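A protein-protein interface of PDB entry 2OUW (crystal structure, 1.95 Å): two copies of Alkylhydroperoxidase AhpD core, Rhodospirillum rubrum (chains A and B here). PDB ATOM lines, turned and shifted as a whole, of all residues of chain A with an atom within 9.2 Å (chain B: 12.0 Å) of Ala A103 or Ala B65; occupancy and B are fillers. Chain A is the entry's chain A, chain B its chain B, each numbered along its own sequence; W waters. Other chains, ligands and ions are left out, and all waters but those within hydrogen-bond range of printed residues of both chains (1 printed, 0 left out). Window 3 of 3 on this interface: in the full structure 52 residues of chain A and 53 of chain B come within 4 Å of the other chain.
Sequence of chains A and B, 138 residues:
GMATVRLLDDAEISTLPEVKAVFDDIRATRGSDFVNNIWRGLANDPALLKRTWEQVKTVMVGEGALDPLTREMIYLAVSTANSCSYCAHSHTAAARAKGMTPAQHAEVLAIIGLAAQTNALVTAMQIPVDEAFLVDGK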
ATOM      1  N   LEU A  69      20.278  27.872  29.764  1.00  0.00           N
ATOM      2  CA  LEU A  69      19.108  27.500  30.545  1.00  0.00           C
ATOM      3  C   LEU A  69      18.228  26.543  29.761  1.00  0.00           C
ATOM      4  O   LEU A  69      17.759  25.559  30.300  1.00  0.00           O
ATOM      5  CB  LEU A  69      18.302  28.744  30.973  1.00  0.00           C
ATOM      6  CG  LEU A  69      17.014  28.442  31.756  1.00  0.00           C
ATOM      7  CD1 LEU A  69      17.302  27.563  32.994  1.00  0.00           C
ATOM      8  CD2 LEU A  69      16.326  29.724  32.166  1.00  0.00           C
ATOM      9  N   THR A  70      18.009  26.825  28.482  1.00  0.00           N
ATOM     10  CA  THR A  70      17.169  25.957  27.645  1.00  0.00           C
ATOM     11  C   THR A  70      17.805  24.583  27.628  1.00  0.00           C
ATOM     12  O   THR A  70      17.121  23.584  27.774  1.00  0.00           O
ATOM     13  CB  THR A  70      17.037  26.485  26.207  1.00  0.00           C
ATOM     14  OG1 THR A  70      16.554  27.821  26.242  1.00  0.00           O
ATOM     15  CG2 THR A  70      16.061  25.649  25.365  1.00  0.00           C
ATOM     16  N   MET A  73      17.067  22.800  30.882  1.00  0.00           N
ATOM     17  CA  MET A  73      15.670  22.364  31.000  1.00  0.00           C
ATOM     18  C   MET A  73      15.340  21.145  30.152  1.00  0.00           C
ATOM     19  O   MET A  73      14.573  20.290  30.555  1.00  0.00           O
ATOM     20  CB  MET A  73      14.732  23.503  30.636  1.00  0.00           C
ATOM     21  CG  MET A  73      14.844  24.654  31.589  1.00  0.00           C
ATOM     22  SD  MET A  73      13.630  26.168  31.288  1.00  0.00           S
ATOM     23  CE  MET A  73      13.514  26.035  29.611  1.00  0.00           C
ATOM     24  N   ARG A  96      18.101  26.162  38.116  1.00  0.00           N
ATOM     25  CA  ARG A  96      17.931  27.305  39.014  1.00  0.00           C
ATOM     26  C   ARG A  96      19.171  28.168  39.013  1.00  0.00           C
ATOM     27  O   ARG A  96      19.078  29.398  38.920  1.00  0.00           O
ATOM     28  CB  ARG A  96      17.661  26.843  40.437  1.00  0.00           C
ATOM     29  CG  ARG A  96      16.309  26.213  40.585  1.00  0.00           C
ATOM     30  CD  ARG A  96      15.834  26.216  42.025  1.00  0.00           C
ATOM     31  NE  ARG A  96      14.506  25.603  42.100  1.00  0.00           N
ATOM     32  CZ  ARG A  96      14.211  24.451  42.698  1.00  0.00           C
ATOM     33  NH1 ARG A  96      15.140  23.758  43.359  1.00  0.00           N
ATOM     34  NH2 ARG A  96      12.955  24.011  42.665  1.00  0.00           N
ATOM     35  N   GLY A  99      19.314  30.361  36.255  1.00  0.00           N
ATOM     36  CA  GLY A  99      18.235  31.361  36.198  1.00  0.00           C
ATOM     37  C   GLY A  99      16.804  30.896  35.954  1.00  0.00           C
ATOM     38  O   GLY A  99      15.932  31.734  35.735  1.00  0.00           O
ATOM     39  N   MET A 100      16.539  29.579  35.990  1.00  0.00           N
ATOM     40  CA  MET A 100      15.153  29.079  35.939  1.00  0.00           C
ATOM     41  C   MET A 100      14.346  29.658  37.090  1.00  0.00           C
ATOM     42  O   MET A 100      14.738  29.567  38.256  1.00  0.00           O
ATOM     43  CB  MET A 100      15.070  27.550  35.968  1.00  0.00           C
ATOM     44  CG  MET A 100      13.653  27.018  35.851  1.00  0.00           C
ATOM     45  SD  MET A 100      13.578  25.102  35.765  1.00  0.00           S
ATOM     46  CE  MET A 100      14.090  24.846  37.718  1.00  0.00           C
ATOM     47  N   THR A 101      13.239  30.294  36.738  1.00  0.00           N
ATOM     48  CA  THR A 101      12.353  30.930  37.693  1.00  0.00           C
ATOM     49  C   THR A 101      11.241  29.934  38.061  1.00  0.00           C
ATOM     50  O   THR A 101      11.019  28.984  37.334  1.00  0.00           O
ATOM     51  CB  THR A 101      11.690  32.152  37.038  1.00  0.00           C
ATOM     52  OG1 THR A 101      10.888  31.696  35.955  1.00  0.00           O
ATOM     53  CG2 THR A 101      12.736  33.105  36.481  1.00  0.00           C
ATOM     54  N   PRO A 102      10.532  30.165  39.190  1.00  0.00           N
ATOM     55  CA  PRO A 102       9.330  29.392  39.514  1.00  0.00           C
ATOM     56  C   PRO A 102       8.395  29.203  38.336  1.00  0.00           C
ATOM     57  O   PRO A 102       7.912  28.094  38.078  1.00  0.00           O
ATOM     58  CB  PRO A 102       8.682  30.223  40.610  1.00  0.00           C
ATOM     59  CG  PRO A 102       9.831  30.811  41.322  1.00  0.00           C
ATOM     60  CD  PRO A 102      10.875  31.100  40.268  1.00  0.00           C
ATOM     61  N   ALA A 103       8.161  30.273  37.587  1.00  0.00           N
ATOM     62  CA  ALA A 103       7.194  30.221  36.495  1.00  0.00           C
ATOM     63  C   ALA A 103       7.609  29.252  35.399  1.00  0.00           C
ATOM     64  O   ALA A 103       6.810  28.486  34.881  1.00  0.00           O
ATOM     65  CB  ALA A 103       6.987  31.623  35.918  1.00  0.00           C
ATOM     66  N   GLN A 104       8.883  29.312  35.044  1.00  0.00           N
ATOM     67  CA  GLN A 104       9.481  28.398  34.042  1.00  0.00           C
ATOM     68  C   GLN A 104       9.482  26.915  34.490  1.00  0.00           C
ATOM     69  O   GLN A 104       9.207  26.008  33.703  1.00  0.00           O
ATOM     70  CB  GLN A 104      10.916  28.849  33.785  1.00  0.00           C
ATOM     71  CG  GLN A 104      11.013  30.214  33.131  1.00  0.00           C
ATOM     72  CD  GLN A 104      12.431  30.689  32.993  1.00  0.00           C
ATOM     73  OE1 GLN A 104      13.232  30.593  33.927  1.00  0.00           O
ATOM     74  NE2 GLN A 104      12.756  31.216  31.830  1.00  0.00           N
ATOM     75  N   HIS A 105       9.792  26.692  35.765  1.00  0.00           N
ATOM     76  CA  HIS A 105       9.814  25.352  36.362  1.00  0.00           C
ATOM     77  C   HIS A 105       8.444  24.691  36.316  1.00  0.00           C
ATOM     78  O   HIS A 105       8.316  23.496  36.078  1.00  0.00           O
ATOM     79  CB  HIS A 105      10.251  25.488  37.813  1.00  0.00           C
ATOM     80  CG  HIS A 105      10.589  24.192  38.485  1.00  0.00           C
ATOM     81  ND1 HIS A 105      10.737  24.092  39.854  1.00  0.00           N
ATOM     82  CD2 HIS A 105      10.784  22.952  37.992  1.00  0.00           C
ATOM     83  CE1 HIS A 105      11.046  22.848  40.168  1.00  0.00           C
ATOM     84  NE2 HIS A 105      11.073  22.133  39.053  1.00  0.00           N
ATOM     85  N   ALA A 106       7.412  25.496  36.541  1.00  0.00           N
ATOM     86  CA  ALA A 106       6.048  25.027  36.552  1.00  0.00           C
ATOM     87  C   ALA A 106       5.636  24.581  35.164  1.00  0.00           C
ATOM     88  O   ALA A 106       4.934  23.583  35.035  1.00  0.00           O
ATOM     89  CB  ALA A 106       5.152  26.113  37.025  1.00  0.00           C
ATOM     90  N   GLU A 107       6.076  25.311  34.139  1.00  0.00           N
ATOM     91  CA  GLU A 107       5.739  24.975  32.756  1.00  0.00           C
ATOM     92  C   GLU A 107       6.510  23.761  32.250  1.00  0.00           C
ATOM     93  O   GLU A 107       6.005  22.978  31.442  1.00  0.00           O
ATOM     94  CB  GLU A 107       5.988  26.176  31.837  1.00  0.00           C
ATOM     95  CG  GLU A 107       5.799  25.891  30.331  1.00  0.00           C
ATOM     96  CD  GLU A 107       4.371  25.528  29.959  1.00  0.00           C
ATOM     97  OE1 GLU A 107       3.446  25.803  30.760  1.00  0.00           O
ATOM     98  OE2 GLU A 107       4.164  24.995  28.844  1.00  0.00           O
ATOM     99  N   VAL A 108       7.744  23.604  32.688  1.00  0.00           N
ATOM    100  CA  VAL A 108       8.530  22.414  32.366  1.00  0.00           C
ATOM    101  C   VAL A 108       7.837  21.160  32.936  1.00  0.00           C
ATOM    102  O   VAL A 108       7.650  20.159  32.237  1.00  0.00           O
ATOM    103  CB  VAL A 108       9.990  22.534  32.914  1.00  0.00           C
ATOM    104  CG1 VAL A 108      10.783  21.227  32.769  1.00  0.00           C
ATOM    105  CG2 VAL A 108      10.735  23.700  32.253  1.00  0.00           C
ATOM    106  N   LEU A 109       7.433  21.233  34.198  1.00  0.00           N
ATOM    107  CA  LEU A 109       6.739  20.132  34.840  1.00  0.00           C
ATOM    108  C   LEU A 109       5.443  19.817  34.097  1.00  0.00           C
ATOM    109  O   LEU A 109       5.141  18.639  33.822  1.00  0.00           O
ATOM    110  CB  LEU A 109       6.455  20.477  36.299  1.00  0.00           C
ATOM    111  CG  LEU A 109       7.632  20.563  37.236  1.00  0.00           C
ATOM    112  CD1 LEU A 109       7.144  21.000  38.625  1.00  0.00           C
ATOM    113  CD2 LEU A 109       8.301  19.272  37.346  1.00  0.00           C
ATOM    114  N   ALA A 110       4.708  20.867  33.705  1.00  0.00           N
ATOM    115  CA  ALA A 110       3.454  20.702  32.951  1.00  0.00           C
ATOM    116  C   ALA A 110       3.682  20.040  31.595  1.00  0.00           C
ATOM    117  O   ALA A 110       2.943  19.152  31.194  1.00  0.00           O
ATOM    118  CB  ALA A 110       2.744  22.057  32.794  1.00  0.00           C
ATOM    119  N   ILE A 111       4.748  20.420  30.908  1.00  0.00           N
ATOM    120  CA  ILE A 111       5.074  19.779  29.664  1.00  0.00           C
ATOM    121  C   ILE A 111       5.488  18.304  29.856  1.00  0.00           C
ATOM    122  O   ILE A 111       5.115  17.440  29.072  1.00  0.00           O
ATOM    123  CB  ILE A 111       6.186  20.542  28.933  1.00  0.00           C
ATOM    124  CG1 ILE A 111       5.675  21.924  28.521  1.00  0.00           C
ATOM    125  CG2 ILE A 111       6.654  19.750  27.741  1.00  0.00           C
ATOM    126  CD1 ILE A 111       6.786  22.885  28.084  1.00  0.00           C
ATOM    127  N   LYS B  57      -3.829  22.310  24.437  1.00  0.00           N
ATOM    128  CA  LYS B  57      -4.111  23.703  24.102  1.00  0.00           C
ATOM    129  C   LYS B  57      -3.644  24.626  25.236  1.00  0.00           C
ATOM    130  O   LYS B  57      -2.991  25.637  24.985  1.00  0.00           O
ATOM    131  CB  LYS B  57      -5.607  23.878  23.796  1.00  0.00           C
ATOM    132  CG  LYS B  57      -5.964  25.153  23.057  1.00  0.00           C
ATOM    133  CD  LYS B  57      -7.474  25.346  22.974  1.00  0.00           C
ATOM    134  CE  LYS B  57      -7.850  26.801  22.665  1.00  0.00           C
ATOM    135  NZ  LYS B  57      -7.420  27.275  21.309  1.00  0.00           N
ATOM    136  N   THR B  58      -3.923  24.266  26.487  1.00  0.00           N
ATOM    137  CA  THR B  58      -3.540  25.105  27.627  1.00  0.00           C
ATOM    138  C   THR B  58      -2.043  25.197  27.846  1.00  0.00           C
ATOM    139  O   THR B  58      -1.517  26.270  28.144  1.00  0.00           O
ATOM    140  CB  THR B  58      -4.152  24.573  28.936  1.00  0.00           C
ATOM    141  OG1 THR B  58      -5.574  24.698  28.868  1.00  0.00           O
ATOM    142  CG2 THR B  58      -3.639  25.338  30.168  1.00  0.00           C
ATOM    143  N   VAL B  59      -1.365  24.063  27.738  1.00  0.00           N
ATOM    144  CA  VAL B  59       0.057  23.975  28.043  1.00  0.00           C
ATOM    145  C   VAL B  59       0.938  24.458  26.905  1.00  0.00           C
ATOM    146  O   VAL B  59       1.932  25.116  27.149  1.00  0.00           O
ATOM    147  CB  VAL B  59       0.423  22.530  28.463  1.00  0.00           C
ATOM    148  CG1 VAL B  59       1.950  22.352  28.642  1.00  0.00           C
ATOM    149  CG2 VAL B  59      -0.287  22.196  29.747  1.00  0.00           C
ATOM    150  N   MET B  60       0.557  24.164  25.666  1.00  0.00           N
ATOM    151  CA  MET B  60       1.430  24.355  24.511  1.00  0.00           C
ATOM    152  C   MET B  60       1.092  25.573  23.662  1.00  0.00           C
ATOM    153  O   MET B  60       1.846  25.895  22.741  1.00  0.00           O
ATOM    154  CB  MET B  60       1.354  23.123  23.600  1.00  0.00           C
ATOM    155  CG  MET B  60       1.707  21.812  24.304  1.00  0.00           C
ATOM    156  SD  MET B  60       3.568  21.871  24.906  1.00  0.00           S
ATOM    157  CE  MET B  60       4.256  21.651  23.069  1.00  0.00           C
ATOM    158  N   VAL B  61      -0.030  26.233  23.961  1.00  0.00           N
ATOM    159  CA  VAL B  61      -0.522  27.368  23.176  1.00  0.00           C
ATOM    160  C   VAL B  61      -0.792  28.571  24.063  1.00  0.00           C
ATOM    161  O   VAL B  61      -1.362  28.475  25.154  1.00  0.00           O
ATOM    162  CB  VAL B  61      -1.817  27.002  22.390  1.00  0.00           C
ATOM    163  CG1 VAL B  61      -2.244  28.136  21.478  1.00  0.00           C
ATOM    164  CG2 VAL B  61      -1.617  25.721  21.585  1.00  0.00           C
ATOM    165  N   GLY B  62      -0.368  29.725  23.579  1.00  0.00           N
ATOM    166  CA  GLY B  62      -0.621  30.980  24.272  1.00  0.00           C
ATOM    167  C   GLY B  62       0.601  31.465  25.008  1.00  0.00           C
ATOM    168  O   GLY B  62       1.611  30.755  25.066  1.00  0.00           O
ATOM    169  N   GLU B  63       0.512  32.679  25.555  1.00  0.00           N
ATOM    170  CA  GLU B  63       1.606  33.258  26.327  1.00  0.00           C
ATOM    171  C   GLU B  63       1.855  32.376  27.563  1.00  0.00           C
ATOM    172  O   GLU B  63       0.932  31.754  28.116  1.00  0.00           O
ATOM    173  CB  GLU B  63       1.308  34.717  26.723  1.00  0.00           C
ATOM    174  N   GLY B  64       3.116  32.316  27.968  1.00  0.00           N
ATOM    175  CA  GLY B  64       3.548  31.440  29.040  1.00  0.00           C
ATOM    176  C   GLY B  64       5.018  31.693  29.279  1.00  0.00           C
ATOM    177  O   GLY B  64       5.619  32.532  28.604  1.00  0.00           O
ATOM    178  N   ALA B  65       5.604  30.968  30.228  1.00  0.00           N
ATOM    179  CA  ALA B  65       6.947  31.289  30.706  1.00  0.00           C
ATOM    180  C   ALA B  65       8.054  30.903  29.710  1.00  0.00           C
ATOM    181  O   ALA B  65       9.197  31.409  29.810  1.00  0.00           O
ATOM    182  CB  ALA B  65       7.188  30.633  32.065  1.00  0.00           C
ATOM    183  N   LEU B  66       7.704  30.042  28.755  1.00  0.00           N
ATOM    184  CA  LEU B  66       8.658  29.502  27.788  1.00  0.00           C
ATOM    185  C   LEU B  66       8.118  29.739  26.392  1.00  0.00           C
ATOM    186  O   LEU B  66       6.924  29.647  26.201  1.00  0.00           O
ATOM    187  CB  LEU B  66       8.808  27.971  27.965  1.00  0.00           C
ATOM    188  CG  LEU B  66       9.271  27.389  29.300  1.00  0.00           C
ATOM    189  CD1 LEU B  66       9.367  25.890  29.170  1.00  0.00           C
ATOM    190  CD2 LEU B  66      10.603  27.995  29.781  1.00  0.00           C
ATOM    191  N   ASP B  67       8.973  29.986  25.400  1.00  0.00           N
ATOM    192  CA  ASP B  67       8.439  30.195  24.042  1.00  0.00           C
ATOM    193  C   ASP B  67       7.993  28.874  23.415  1.00  0.00           C
ATOM    194  O   ASP B  67       8.395  27.808  23.867  1.00  0.00           O
ATOM    195  CB  ASP B  67       9.379  31.031  23.147  1.00  0.00           C
ATOM    196  CG  ASP B  67      10.725  30.379  22.894  1.00  0.00           C
ATOM    197  OD1 ASP B  67      10.794  29.153  22.720  1.00  0.00           O
ATOM    198  OD2 ASP B  67      11.727  31.130  22.822  1.00  0.00           O
ATOM    199  N   PRO B  68       7.116  28.940  22.402  1.00  0.00           N
ATOM    200  CA  PRO B  68       6.561  27.737  21.818  1.00  0.00           C
ATOM    201  C   PRO B  68       7.573  26.741  21.306  1.00  0.00           C
ATOM    202  O   PRO B  68       7.329  25.552  21.399  1.00  0.00           O
ATOM    203  CB  PRO B  68       5.705  28.282  20.664  1.00  0.00           C
ATOM    204  CG  PRO B  68       5.281  29.586  21.141  1.00  0.00           C
ATOM    205  CD  PRO B  68       6.529  30.139  21.773  1.00  0.00           C
ATOM    206  N   LEU B  69       8.683  27.217  20.746  1.00  0.00           N
ATOM    207  CA  LEU B  69       9.705  26.315  20.221  1.00  0.00           C
ATOM    208  C   LEU B  69      10.372  25.577  21.365  1.00  0.00           C
ATOM    209  O   LEU B  69      10.601  24.386  21.293  1.00  0.00           O
ATOM    210  CB  LEU B  69      10.756  27.076  19.393  1.00  0.00           C
ATOM    211  CG  LEU B  69      11.929  26.227  18.880  1.00  0.00           C
ATOM    212  CD1 LEU B  69      11.424  25.002  18.115  1.00  0.00           C
ATOM    213  CD2 LEU B  69      12.855  27.037  18.018  1.00  0.00           C
ATOM    214  N   THR B  70      10.696  26.296  22.429  1.00  0.00           N
ATOM    215  CA  THR B  70      11.292  25.672  23.595  1.00  0.00           C
ATOM    216  C   THR B  70      10.383  24.560  24.134  1.00  0.00           C
ATOM    217  O   THR B  70      10.840  23.456  24.404  1.00  0.00           O
ATOM    218  CB  THR B  70      11.603  26.746  24.661  1.00  0.00           C
ATOM    219  OG1 THR B  70      12.468  27.741  24.076  1.00  0.00           O
ATOM    220  CG2 THR B  70      12.278  26.148  25.877  1.00  0.00           C
ATOM    221  N   ARG B  71       9.091  24.838  24.232  1.00  0.00           N
ATOM    222  CA  ARG B  71       8.106  23.827  24.666  1.00  0.00           C
ATOM    223  C   ARG B  71       8.102  22.584  23.815  1.00  0.00           C
ATOM    224  O   ARG B  71       8.010  21.484  24.336  1.00  0.00           O
ATOM    225  CB  ARG B  71       6.702  24.397  24.656  1.00  0.00           C
ATOM    226  CG  ARG B  71       6.517  25.600  25.548  1.00  0.00           C
ATOM    227  CD  ARG B  71       5.136  26.174  25.324  1.00  0.00           C
ATOM    228  NE  ARG B  71       5.009  27.447  26.009  1.00  0.00           N
ATOM    229  CZ  ARG B  71       3.940  28.227  25.915  1.00  0.00           C
ATOM    230  NH1 ARG B  71       2.915  27.853  25.172  1.00  0.00           N
ATOM    231  NH2 ARG B  71       3.890  29.365  26.580  1.00  0.00           N
ATOM    232  N   GLU B  72       8.190  22.753  22.494  1.00  0.00           N
ATOM    233  CA  GLU B  72       8.242  21.597  21.602  1.00  0.00           C
ATOM    234  C   GLU B  72       9.543  20.811  21.741  1.00  0.00           C
ATOM    235  O   GLU B  72       9.552  19.590  21.596  1.00  0.00           O
ATOM    236  CB  GLU B  72       8.073  21.992  20.133  1.00  0.00           C
ATOM    237  CG  GLU B  72       6.648  22.081  19.646  1.00  0.00           C
ATOM    238  CD  GLU B  72       5.801  20.828  19.873  1.00  0.00           C
ATOM    239  OE1 GLU B  72       6.322  19.690  19.894  1.00  0.00           O
ATOM    240  OE2 GLU B  72       4.581  21.008  20.018  1.00  0.00           O
ATOM    241  N   MET B  73      10.649  21.489  22.024  1.00  0.00           N
ATOM    242  CA  MET B  73      11.928  20.771  22.139  1.00  0.00           C
ATOM    243  C   MET B  73      11.925  19.935  23.412  1.00  0.00           C
ATOM    244  O   MET B  73      12.393  18.807  23.425  1.00  0.00           O
ATOM    245  CB  MET B  73      13.090  21.753  22.112  1.00  0.00           C
ATOM    246  CG  MET B  73      13.184  22.484  20.784  1.00  0.00           C
ATOM    247  SD  MET B  73      14.711  23.671  20.627  1.00  0.00           S
ATOM    248  CE  MET B  73      15.058  24.128  22.487  1.00  0.00           C
ATOM    249  N   ILE B  74      11.359  20.479  24.481  1.00  0.00           N
ATOM    250  CA  ILE B  74      11.217  19.709  25.690  1.00  0.00           C
ATOM    251  C   ILE B  74      10.309  18.496  25.416  1.00  0.00           C
ATOM    252  O   ILE B  74      10.653  17.359  25.780  1.00  0.00           O
ATOM    253  CB  ILE B  74      10.642  20.539  26.822  1.00  0.00           C
ATOM    254  CG1 ILE B  74      11.657  21.575  27.302  1.00  0.00           C
ATOM    255  CG2 ILE B  74      10.274  19.652  27.990  1.00  0.00           C
ATOM    256  CD1 ILE B  74      11.040  22.686  28.158  1.00  0.00           C
HETATM  257  O   HOH W   1       4.074  29.144  31.425  1.00  0.00           O
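Of the 17 printed residues of chain A, 6 touch a printed residue of chain B.
Printed residues of chain A that touch a printed residue of chain B: Thr A70, Met A73, Ala A103, Gln A104, Glu A107 and Ile A111.
Hydrophobic or aromatic side chains of chain A within 4 Å of the printed part of chain B: Met A73, Ala A103 and Ile A111.
Hydrophobic or aromatic side chains of chain B within 4 Å of the printed part of chain A: Val B59, Ala B65, Leu B66, Met B73 and Ile B74.
Among the printed residues, 12 pairs touch across the chains.
Among the printed residues, Asp or Glu carboxylates within 4 Å of a Lys or Arg side-chain nitrogen of the other chain: Glu A107 with Arg B71 (3.8 Å).
Among the printed residues, pairs that only touch across the chains: Thr A70 with Thr B70 (3.8 Å), Thr A70 with Met B73 (3.4 Å), Met A73 with Leu B66 (3.5 Å), Met A73 with Thr B70 (3.9 Å), Ala A103 with Ala B65 (3.6 Å), Gln A104 with Ala B65 (3.7 Å), Glu A107 with Leu B66 (3.8 Å), Ile A111 with Val B59 (3.8 Å), Ile A111 with Arg B71 (3.7 Å) and Ile A111 with Ile B74 (3.6 Å).
Water W1 bridges N of Ala B65 (2.7 Å) and OE1 of Glu A107 (3.5 Å).
Printed residues of chain A within 4 Å of Ala B65: Ala A103 (3.6 Å) and Gln A104 (3.7 Å).
No residue of chain B comes within 4 Å of Thr A101.
Of chain B, only Ala B65 (3.7 Å) comes within 4 Å of Gln A104.
No residue of chain B comes within 4 Å of Ala A106.
Of the printed residues of chain A, Leu B66 touches Met A73 (3.5 Å) and Glu A107 (3.8 Å).
Of the printed residues of chain A, Arg B71 touches Glu A107 and Ile A111.
Printed residues of chain A within 4 Å of Val B59: Glu A107 and Ile A111.
Of the printed residues of chain B, Thr A70 touches Thr B70 and Met B73.
Of the printed residues of chain A, Ile B74 touches Ile A111 (3.6 Å).
The nearest residue of chain B that does not touch Ala A103 is Leu B66 (6.2 Å).
The nearest printed residue of chain A that does not touch Ala B65 is Glu A107 (4.6 Å).
NE of Arg B71 is in salt-bridge range of OE2 of Glu A107 (3.8 Å).
The side-chain carboxylate (OE2) of Glu A107 sits close to the backbone carbonyl oxygen (O) of Val B59 (2.8 Å).
The backbone carbonyl oxygen (O) of Gly A99 lies close to the side-chain amide oxygen (OE1) of Gln A104, at 3.4 Å.
The side-chain hydroxyl (OG1) of Thr A101 lies close to the backbone NH (N) of Ala A103, 3.5 Å away.
N of Thr A101 sits at hydrogen-bond distance from OE1 of Gln A104, 2.8 Å away.
O of Gly B62 sits at hydrogen-bond distance from NH2 of Arg B71.
The backbone carbonyl oxygen (O) of Leu B66 lies within hydrogen-bond range of the guanidinium group (NE) of Arg B71 (2.9 Å).
OD1 of Asp B67 sits at hydrogen-bond distance from OG1 of Thr B70 (2.6 Å).
Thr B70 touches its own counterpart, Thr A70.
Thr A70 touches Met B73, and with the chains exchanged Met A73 touches Thr B70.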
